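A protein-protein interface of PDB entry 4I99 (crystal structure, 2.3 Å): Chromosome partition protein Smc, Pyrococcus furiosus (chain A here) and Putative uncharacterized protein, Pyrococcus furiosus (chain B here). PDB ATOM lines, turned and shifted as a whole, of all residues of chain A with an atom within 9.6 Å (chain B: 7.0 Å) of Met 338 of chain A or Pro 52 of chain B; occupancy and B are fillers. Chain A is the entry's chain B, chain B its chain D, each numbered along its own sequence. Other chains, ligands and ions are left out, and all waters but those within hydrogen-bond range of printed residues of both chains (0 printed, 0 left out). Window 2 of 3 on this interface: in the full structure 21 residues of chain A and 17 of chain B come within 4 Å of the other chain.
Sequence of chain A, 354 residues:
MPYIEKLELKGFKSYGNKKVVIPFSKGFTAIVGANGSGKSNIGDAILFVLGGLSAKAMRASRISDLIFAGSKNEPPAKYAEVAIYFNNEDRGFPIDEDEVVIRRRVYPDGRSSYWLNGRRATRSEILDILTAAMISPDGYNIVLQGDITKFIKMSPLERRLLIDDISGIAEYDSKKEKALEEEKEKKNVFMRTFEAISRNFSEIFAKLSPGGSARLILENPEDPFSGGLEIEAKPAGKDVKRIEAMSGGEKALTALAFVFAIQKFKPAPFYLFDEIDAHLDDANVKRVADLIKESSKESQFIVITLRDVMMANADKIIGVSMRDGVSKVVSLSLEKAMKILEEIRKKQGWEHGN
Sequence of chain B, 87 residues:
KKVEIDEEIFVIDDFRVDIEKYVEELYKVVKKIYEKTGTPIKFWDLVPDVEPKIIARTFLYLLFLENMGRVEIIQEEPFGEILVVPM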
ATOM      1  N   LYS A 293      10.513  11.904  26.272  1.00  0.00           N
ATOM      2  CA  LYS A 293      10.402  12.373  24.894  1.00  0.00           C
ATOM      3  C   LYS A 293      11.544  13.321  24.566  1.00  0.00           C
ATOM      4  O   LYS A 293      12.253  13.140  23.576  1.00  0.00           O
ATOM      5  CB  LYS A 293       9.072  13.091  24.659  1.00  0.00           C
ATOM      6  CG  LYS A 293       7.932  12.167  24.247  1.00  0.00           C
ATOM      7  CD  LYS A 293       6.729  12.940  23.680  1.00  0.00           C
ATOM      8  CE  LYS A 293       6.094  13.881  24.713  1.00  0.00           C
ATOM      9  NZ  LYS A 293       4.841  14.530  24.208  1.00  0.00           N
ATOM     10  N   ASP A 308      -1.436   4.178  30.740  1.00  0.00           N
ATOM     11  CA  ASP A 308      -1.927   4.808  29.506  1.00  0.00           C
ATOM     12  C   ASP A 308      -1.217   6.092  29.153  1.00  0.00           C
ATOM     13  O   ASP A 308      -0.913   6.334  27.985  1.00  0.00           O
ATOM     14  CB  ASP A 308      -3.421   5.110  29.615  1.00  0.00           C
ATOM     15  CG  ASP A 308      -4.212   3.949  30.183  1.00  0.00           C
ATOM     16  OD1 ASP A 308      -4.204   2.849  29.573  1.00  0.00           O
ATOM     17  OD2 ASP A 308      -4.839   4.141  31.252  1.00  0.00           O
ATOM     18  N   VAL A 309      -0.974   6.924  30.160  1.00  0.00           N
ATOM     19  CA  VAL A 309      -0.303   8.191  29.948  1.00  0.00           C
ATOM     20  C   VAL A 309       1.086   7.972  29.365  1.00  0.00           C
ATOM     21  O   VAL A 309       1.547   8.745  28.522  1.00  0.00           O
ATOM     22  CB  VAL A 309      -0.163   8.972  31.265  1.00  0.00           C
ATOM     23  CG1 VAL A 309       0.586  10.286  31.023  1.00  0.00           C
ATOM     24  CG2 VAL A 309      -1.537   9.237  31.856  1.00  0.00           C
ATOM     25  N   MET A 310       1.755   6.912  29.807  1.00  0.00           N
ATOM     26  CA  MET A 310       3.099   6.625  29.324  1.00  0.00           C
ATOM     27  C   MET A 310       3.145   6.144  27.862  1.00  0.00           C
ATOM     28  O   MET A 310       3.956   6.632  27.067  1.00  0.00           O
ATOM     29  CB  MET A 310       3.770   5.597  30.237  1.00  0.00           C
ATOM     30  CG  MET A 310       5.222   5.288  29.883  1.00  0.00           C
ATOM     31  SD  MET A 310       6.470   6.785  30.053  1.00  0.00           S
ATOM     32  CE  MET A 310       6.697   6.752  31.987  1.00  0.00           C
ATOM     33  N   MET A 311       2.280   5.202  27.498  1.00  0.00           N
ATOM     34  CA  MET A 311       2.295   4.691  26.130  1.00  0.00           C
ATOM     35  C   MET A 311       1.810   5.710  25.116  1.00  0.00           C
ATOM     36  O   MET A 311       2.276   5.734  23.973  1.00  0.00           O
ATOM     37  CB  MET A 311       1.464   3.419  26.021  1.00  0.00           C
ATOM     38  CG  MET A 311      -0.010   3.606  26.227  1.00  0.00           C
ATOM     39  SD  MET A 311      -0.925   1.927  25.917  1.00  0.00           S
ATOM     40  CE  MET A 311      -0.666   1.818  24.012  1.00  0.00           C
ATOM     41  N   ALA A 312       0.886   6.562  25.543  1.00  0.00           N
ATOM     42  CA  ALA A 312       0.337   7.596  24.678  1.00  0.00           C
ATOM     43  C   ALA A 312       1.396   8.599  24.209  1.00  0.00           C
ATOM     44  O   ALA A 312       1.225   9.244  23.169  1.00  0.00           O
ATOM     45  CB  ALA A 312      -0.801   8.335  25.409  1.00  0.00           C
ATOM     46  N   ASN A 313       2.487   8.727  24.962  1.00  0.00           N
ATOM     47  CA  ASN A 313       3.546   9.674  24.614  1.00  0.00           C
ATOM     48  C   ASN A 313       4.679   9.082  23.786  1.00  0.00           C
ATOM     49  O   ASN A 313       5.631   9.781  23.437  1.00  0.00           O
ATOM     50  CB  ASN A 313       4.113  10.310  25.891  1.00  0.00           C
ATOM     51  CG  ASN A 313       3.196  11.392  26.460  1.00  0.00           C
ATOM     52  OD1 ASN A 313       3.249  12.555  26.042  1.00  0.00           O
ATOM     53  ND2 ASN A 313       2.337  11.008  27.400  1.00  0.00           N
ATOM     54  N   ALA A 314       4.562   7.803  23.446  1.00  0.00           N
ATOM     55  CA  ALA A 314       5.595   7.118  22.676  1.00  0.00           C
ATOM     56  C   ALA A 314       5.583   7.412  21.173  1.00  0.00           C
ATOM     57  O   ALA A 314       4.545   7.753  20.601  1.00  0.00           O
ATOM     58  CB  ALA A 314       5.481   5.616  22.904  1.00  0.00           C
ATOM     59  N   ASP A 315       6.753   7.288  20.545  1.00  0.00           N
ATOM     60  CA  ASP A 315       6.875   7.485  19.105  1.00  0.00           C
ATOM     61  C   ASP A 315       6.347   6.208  18.468  1.00  0.00           C
ATOM     62  O   ASP A 315       5.560   6.246  17.530  1.00  0.00           O
ATOM     63  CB  ASP A 315       8.334   7.681  18.694  1.00  0.00           C
ATOM     64  CG  ASP A 315       8.954   8.924  19.302  1.00  0.00           C
ATOM     65  OD1 ASP A 315       8.377  10.017  19.123  1.00  0.00           O
ATOM     66  OD2 ASP A 315      10.019   8.812  19.952  1.00  0.00           O
ATOM     67  N   ILE A 317       5.064   1.890  19.306  1.00  0.00           N
ATOM     68  CA  ILE A 317       4.583   0.970  20.315  1.00  0.00           C
ATOM     69  C   ILE A 317       4.756  -0.490  19.930  1.00  0.00           C
ATOM     70  O   ILE A 317       4.481  -0.879  18.792  1.00  0.00           O
ATOM     71  CB  ILE A 317       3.102   1.201  20.587  1.00  0.00           C
ATOM     72  CG1 ILE A 317       2.882   2.619  21.107  1.00  0.00           C
ATOM     73  CG2 ILE A 317       2.606   0.182  21.589  1.00  0.00           C
ATOM     74  CD1 ILE A 317       1.429   3.025  21.201  1.00  0.00           C
ATOM     75  N   LEU A 332       3.580  -1.041  16.044  1.00  0.00           N
ATOM     76  CA  LEU A 332       2.763   0.058  15.558  1.00  0.00           C
ATOM     77  C   LEU A 332       3.522   1.380  15.680  1.00  0.00           C
ATOM     78  O   LEU A 332       4.065   1.703  16.738  1.00  0.00           O
ATOM     79  CB  LEU A 332       1.473   0.134  16.373  1.00  0.00           C
ATOM     80  CG  LEU A 332       0.586   1.358  16.162  1.00  0.00           C
ATOM     81  CD1 LEU A 332       0.005   1.316  14.759  1.00  0.00           C
ATOM     82  CD2 LEU A 332      -0.520   1.378  17.219  1.00  0.00           C
ATOM     83  N   SER A 333       3.562   2.141  14.593  1.00  0.00           N
ATOM     84  CA  SER A 333       4.250   3.426  14.603  1.00  0.00           C
ATOM     85  C   SER A 333       3.242   4.570  14.586  1.00  0.00           C
ATOM     86  O   SER A 333       2.604   4.818  13.568  1.00  0.00           O
ATOM     87  CB  SER A 333       5.175   3.542  13.393  1.00  0.00           C
ATOM     88  OG  SER A 333       5.829   4.798  13.377  1.00  0.00           O
ATOM     89  N   LEU A 334       3.091   5.259  15.713  1.00  0.00           N
ATOM     90  CA  LEU A 334       2.157   6.375  15.790  1.00  0.00           C
ATOM     91  C   LEU A 334       2.596   7.474  14.831  1.00  0.00           C
ATOM     92  O   LEU A 334       1.782   8.277  14.375  1.00  0.00           O
ATOM     93  CB  LEU A 334       2.097   6.927  17.213  1.00  0.00           C
ATOM     94  CG  LEU A 334       1.537   6.002  18.293  1.00  0.00           C
ATOM     95  CD1 LEU A 334       1.402   6.781  19.594  1.00  0.00           C
ATOM     96  CD2 LEU A 334       0.183   5.459  17.865  1.00  0.00           C
ATOM     97  N   GLU A 335       3.888   7.498  14.524  1.00  0.00           N
ATOM     98  CA  GLU A 335       4.453   8.486  13.609  1.00  0.00           C
ATOM     99  C   GLU A 335       3.862   8.327  12.201  1.00  0.00           C
ATOM    100  O   GLU A 335       3.352   9.286  11.619  1.00  0.00           O
ATOM    101  CB  GLU A 335       5.977   8.327  13.560  1.00  0.00           C
ATOM    102  CG  GLU A 335       6.656   8.389  14.932  1.00  0.00           C
ATOM    103  CD  GLU A 335       8.160   8.152  14.860  1.00  0.00           C
ATOM    104  OE1 GLU A 335       8.571   7.057  14.418  1.00  0.00           O
ATOM    105  OE2 GLU A 335       8.931   9.060  15.245  1.00  0.00           O
ATOM    106  N   LYS A 336       3.931   7.110  11.664  1.00  0.00           N
ATOM    107  CA  LYS A 336       3.404   6.819  10.333  1.00  0.00           C
ATOM    108  C   LYS A 336       1.959   6.328  10.389  1.00  0.00           C
ATOM    109  O   LYS A 336       1.447   5.785   9.411  1.00  0.00           O
ATOM    110  CB  LYS A 336       4.258   5.756   9.624  1.00  0.00           C
ATOM    111  CG  LYS A 336       5.712   6.146   9.346  1.00  0.00           C
ATOM    112  CD  LYS A 336       6.606   5.980  10.574  1.00  0.00           C
ATOM    113  CE  LYS A 336       8.075   6.199  10.224  1.00  0.00           C
ATOM    114  NZ  LYS A 336       8.987   5.922  11.371  1.00  0.00           N
ATOM    115  N   ALA A 337       1.304   6.510  11.532  1.00  0.00           N
ATOM    116  CA  ALA A 337      -0.083   6.077  11.692  1.00  0.00           C
ATOM    117  C   ALA A 337      -1.032   7.266  11.631  1.00  0.00           C
ATOM    118  O   ALA A 337      -2.171   7.140  11.179  1.00  0.00           O
ATOM    119  CB  ALA A 337      -0.256   5.338  13.014  1.00  0.00           C
ATOM    120  N   MET A 338      -0.559   8.422  12.091  1.00  0.00           N
ATOM    121  CA  MET A 338      -1.368   9.632  12.078  1.00  0.00           C
ATOM    122  C   MET A 338      -1.673  10.069  10.648  1.00  0.00           C
ATOM    123  O   MET A 338      -2.722  10.663  10.383  1.00  0.00           O
ATOM    124  CB  MET A 338      -0.649  10.762  12.823  1.00  0.00           C
ATOM    125  CG  MET A 338      -0.756  10.678  14.342  1.00  0.00           C
ATOM    126  SD  MET A 338      -2.556  10.983  15.024  1.00  0.00           S
ATOM    127  CE  MET A 338      -2.380  12.854  15.482  1.00  0.00           C
ATOM    128  N   LYS A 339      -0.759   9.771   9.728  1.00  0.00           N
ATOM    129  CA  LYS A 339      -0.941  10.141   8.330  1.00  0.00           C
ATOM    130  C   LYS A 339      -1.957   9.249   7.623  1.00  0.00           C
ATOM    131  O   LYS A 339      -1.818   8.953   6.438  1.00  0.00           O
ATOM    132  CB  LYS A 339       0.397  10.097   7.589  1.00  0.00           C
ATOM    133  CG  LYS A 339       1.165   8.799   7.742  1.00  0.00           C
ATOM    134  CD  LYS A 339       2.413   8.798   6.868  1.00  0.00           C
ATOM    135  CE  LYS A 339       3.338   9.964   7.197  1.00  0.00           C
ATOM    136  NZ  LYS A 339       4.510  10.020   6.277  1.00  0.00           N
ATOM    137  N   ILE A 340      -2.974   8.820   8.366  1.00  0.00           N
ATOM    138  CA  ILE A 340      -4.040   7.982   7.825  1.00  0.00           C
ATOM    139  C   ILE A 340      -5.377   8.382   8.453  1.00  0.00           C
ATOM    140  O   ILE A 340      -6.223   8.947   7.726  1.00  0.00           O
ATOM    141  CB  ILE A 340      -3.790   6.473   8.103  1.00  0.00           C
ATOM    142  CG1 ILE A 340      -2.632   5.951   7.245  1.00  0.00           C
ATOM    143  CG2 ILE A 340      -5.045   5.672   7.800  1.00  0.00           C
ATOM    144  CD1 ILE A 340      -1.258   6.313   7.754  1.00  0.00           C
ATOM    145  N   TRP B  44      -7.011   0.129  11.069  1.00  0.00           N
ATOM    146  CA  TRP B  44      -7.424   1.494  10.758  1.00  0.00           C
ATOM    147  C   TRP B  44      -8.930   1.716  10.949  1.00  0.00           C
ATOM    148  O   TRP B  44      -9.345   2.707  11.558  1.00  0.00           O
ATOM    149  CB  TRP B  44      -7.025   1.836   9.315  1.00  0.00           C
ATOM    150  CG  TRP B  44      -5.525   1.778   9.024  1.00  0.00           C
ATOM    151  CD1 TRP B  44      -4.936   1.454   7.826  1.00  0.00           C
ATOM    152  CD2 TRP B  44      -4.446   2.087   9.924  1.00  0.00           C
ATOM    153  NE1 TRP B  44      -3.567   1.540   7.928  1.00  0.00           N
ATOM    154  CE2 TRP B  44      -3.239   1.927   9.202  1.00  0.00           C
ATOM    155  CE3 TRP B  44      -4.382   2.485  11.268  1.00  0.00           C
ATOM    156  CZ2 TRP B  44      -1.982   2.150   9.781  1.00  0.00           C
ATOM    157  CZ3 TRP B  44      -3.128   2.708  11.844  1.00  0.00           C
ATOM    158  CH2 TRP B  44      -1.947   2.538  11.097  1.00  0.00           C
ATOM    159  N   ASP B  49     -11.344   8.292  16.836  1.00  0.00           N
ATOM    160  CA  ASP B  49     -10.730   9.598  16.627  1.00  0.00           C
ATOM    161  C   ASP B  49      -9.281   9.440  16.191  1.00  0.00           C
ATOM    162  O   ASP B  49      -8.565   8.584  16.706  1.00  0.00           O
ATOM    163  CB  ASP B  49     -10.799  10.418  17.918  1.00  0.00           C
ATOM    164  CG  ASP B  49     -12.138  10.274  18.626  1.00  0.00           C
ATOM    165  OD1 ASP B  49     -13.185  10.389  17.954  1.00  0.00           O
ATOM    166  OD2 ASP B  49     -12.142  10.049  19.856  1.00  0.00           O
ATOM    167  N   VAL B  50      -8.854  10.262  15.239  1.00  0.00           N
ATOM    168  CA  VAL B  50      -7.482  10.205  14.741  1.00  0.00           C
ATOM    169  C   VAL B  50      -6.502  10.859  15.714  1.00  0.00           C
ATOM    170  O   VAL B  50      -5.741  11.752  15.342  1.00  0.00           O
ATOM    171  CB  VAL B  50      -7.355  10.894  13.360  1.00  0.00           C
ATOM    172  CG1 VAL B  50      -8.045  10.056  12.293  1.00  0.00           C
ATOM    173  CG2 VAL B  50      -7.968  12.284  13.415  1.00  0.00           C
ATOM    174  N   GLU B  51      -6.524  10.397  16.961  1.00  0.00           N
ATOM    175  CA  GLU B  51      -5.648  10.923  18.001  1.00  0.00           C
ATOM    176  C   GLU B  51      -4.761   9.842  18.630  1.00  0.00           C
ATOM    177  O   GLU B  51      -5.193   8.708  18.835  1.00  0.00           O
ATOM    178  CB  GLU B  51      -6.489  11.608  19.081  1.00  0.00           C
ATOM    179  CG  GLU B  51      -6.623  13.114  18.900  1.00  0.00           C
ATOM    180  CD  GLU B  51      -7.922  13.657  19.463  1.00  0.00           C
ATOM    181  OE1 GLU B  51      -8.397  13.123  20.490  1.00  0.00           O
ATOM    182  OE2 GLU B  51      -8.462  14.627  18.881  1.00  0.00           O
ATOM    183  N   PRO B  52      -3.501  10.195  18.946  1.00  0.00           N
ATOM    184  CA  PRO B  52      -2.510   9.299  19.551  1.00  0.00           C
ATOM    185  C   PRO B  52      -3.011   8.495  20.749  1.00  0.00           C
ATOM    186  O   PRO B  52      -2.767   7.295  20.843  1.00  0.00           O
ATOM    187  CB  PRO B  52      -1.381  10.253  19.927  1.00  0.00           C
ATOM    188  CG  PRO B  52      -1.429  11.249  18.809  1.00  0.00           C
ATOM    189  CD  PRO B  52      -2.913  11.525  18.704  1.00  0.00           C
ATOM    190  N   LYS B  53      -3.708   9.160  21.660  1.00  0.00           N
ATOM    191  CA  LYS B  53      -4.230   8.496  22.847  1.00  0.00           C
ATOM    192  C   LYS B  53      -5.264   7.425  22.505  1.00  0.00           C
ATOM    193  O   LYS B  53      -5.298   6.364  23.131  1.00  0.00           O
ATOM    194  CB  LYS B  53      -4.845   9.527  23.793  1.00  0.00           C
ATOM    195  N   ILE B  54      -6.106   7.707  21.512  1.00  0.00           N
ATOM    196  CA  ILE B  54      -7.154   6.771  21.108  1.00  0.00           C
ATOM    197  C   ILE B  54      -6.621   5.622  20.258  1.00  0.00           C
ATOM    198  O   ILE B  54      -7.000   4.469  20.464  1.00  0.00           O
ATOM    199  CB  ILE B  54      -8.295   7.486  20.320  1.00  0.00           C
ATOM    200  CG1 ILE B  54      -8.989   8.529  21.203  1.00  0.00           C
ATOM    201  CG2 ILE B  54      -9.323   6.469  19.857  1.00  0.00           C
ATOM    202  CD1 ILE B  54      -8.169   9.780  21.447  1.00  0.00           C
ATOM    203  N   ILE B  55      -5.753   5.937  19.301  1.00  0.00           N
ATOM    204  CA  ILE B  55      -5.176   4.913  18.438  1.00  0.00           C
ATOM    205  C   ILE B  55      -4.358   3.928  19.277  1.00  0.00           C
ATOM    206  O   ILE B  55      -4.181   2.771  18.895  1.00  0.00           O
ATOM    207  CB  ILE B  55      -4.261   5.535  17.354  1.00  0.00           C
ATOM    208  CG1 ILE B  55      -3.549   4.427  16.569  1.00  0.00           C
ATOM    209  CG2 ILE B  55      -3.247   6.468  18.000  1.00  0.00           C
ATOM    210  CD1 ILE B  55      -2.629   4.935  15.477  1.00  0.00           C
ATOM    211  N   ALA B  56      -3.873   4.395  20.425  1.00  0.00           N
ATOM    212  CA  ALA B  56      -3.078   3.560  21.320  1.00  0.00           C
ATOM    213  C   ALA B  56      -3.966   2.682  22.200  1.00  0.00           C
ATOM    214  O   ALA B  56      -3.621   1.536  22.490  1.00  0.00           O
ATOM    215  CB  ALA B  56      -2.170   4.434  22.187  1.00  0.00           C
ATOM    216  N   ARG B  57      -5.104   3.219  22.626  1.00  0.00           N
ATOM    217  CA  ARG B  57      -6.029   2.456  23.458  1.00  0.00           C
ATOM    218  C   ARG B  57      -6.639   1.336  22.625  1.00  0.00           C
ATOM    219  O   ARG B  57      -6.706   0.192  23.066  1.00  0.00           O
ATOM    220  CB  ARG B  57      -7.128   3.363  24.005  1.00  0.00           C
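O of Val 50 of chain B lies close to SD of Met 338 of chain A, at 3.3 Å.
O of Asp 315 of chain A sits at hydrogen-bond distance from N of Leu 334 of chain A (3.2 Å).
N of Ile 317 of chain A lies within hydrogen-bond range of O of Leu 332 of chain A (2.8 Å).
Among the printed residues, pairs that only touch across the chains: Met 311 of chain A with Ala 56 of chain B (3.3 Å), Ala 337 of chain A with Ile 55 of chain B (3.4 Å), Met 338 of chain A with Pro 52 of chain B (3.5 Å), Leu 334 of chain A with Ile 55 of chain B (3.6 Å), Ala 337 of chain A with Trp 44 of chain B (3.8 Å) and Ile 317 of chain A with Ala 56 of chain B (3.99 Å).
Val 309 of chain A touches none of the printed residues of chain B.
Of the printed residues of chain B, Ile 317 of chain A touches Ala 56.
Of the printed residues of chain B, Ala 337 of chain A touches Trp 44 (3.8 Å) and Ile 55 (3.4 Å).
Met 338 of chain A touches just these residues of chain B: Val 50 (3.3 Å) and Pro 52 (3.5 Å).
Printed residues of chain A within 4 Å of Trp 44 of chain B: Ala 337 (3.8 Å).
Of the printed residues of chain A, Val 50 of chain B touches Met 338.
Of the printed residues of chain A, Pro 52 of chain B touches Met 338 (3.5 Å).
No residue of chain A comes within 4 Å of Lys 53 of chain B.
Of chain A, only Leu 334 and Ala 337 come within 4 Å of Ile 55 of chain B.
Of the printed residues of chain A, Ala 56 of chain B touches Met 311 and Ile 317.
The nearest printed residue of chain A that does not touch Val 50 of chain B is Ile 340 of chain A (5.0 Å).
Printed residues of chain A that touch a printed residue of chain B: Met 311, Ile 317, Leu 334, Ala 337 and Met 338.
Hydrophobic or aromatic side chains of chain A that line the printed part of chain B: Met 311, Ile 317, Leu 334, Ala 337 and Met 338.
Of the 10 printed residues of chain B, 5 touch a printed residue of chain A.
Printed residues of chain B that touch a printed residue of chain A: Trp 44, Val 50, Pro 52, Ile 55 and Ala 56.
Among the printed residues, no Asp or Glu carboxylate lies within 4 Å of a Lys or Arg side-chain nitrogen of the other chain.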
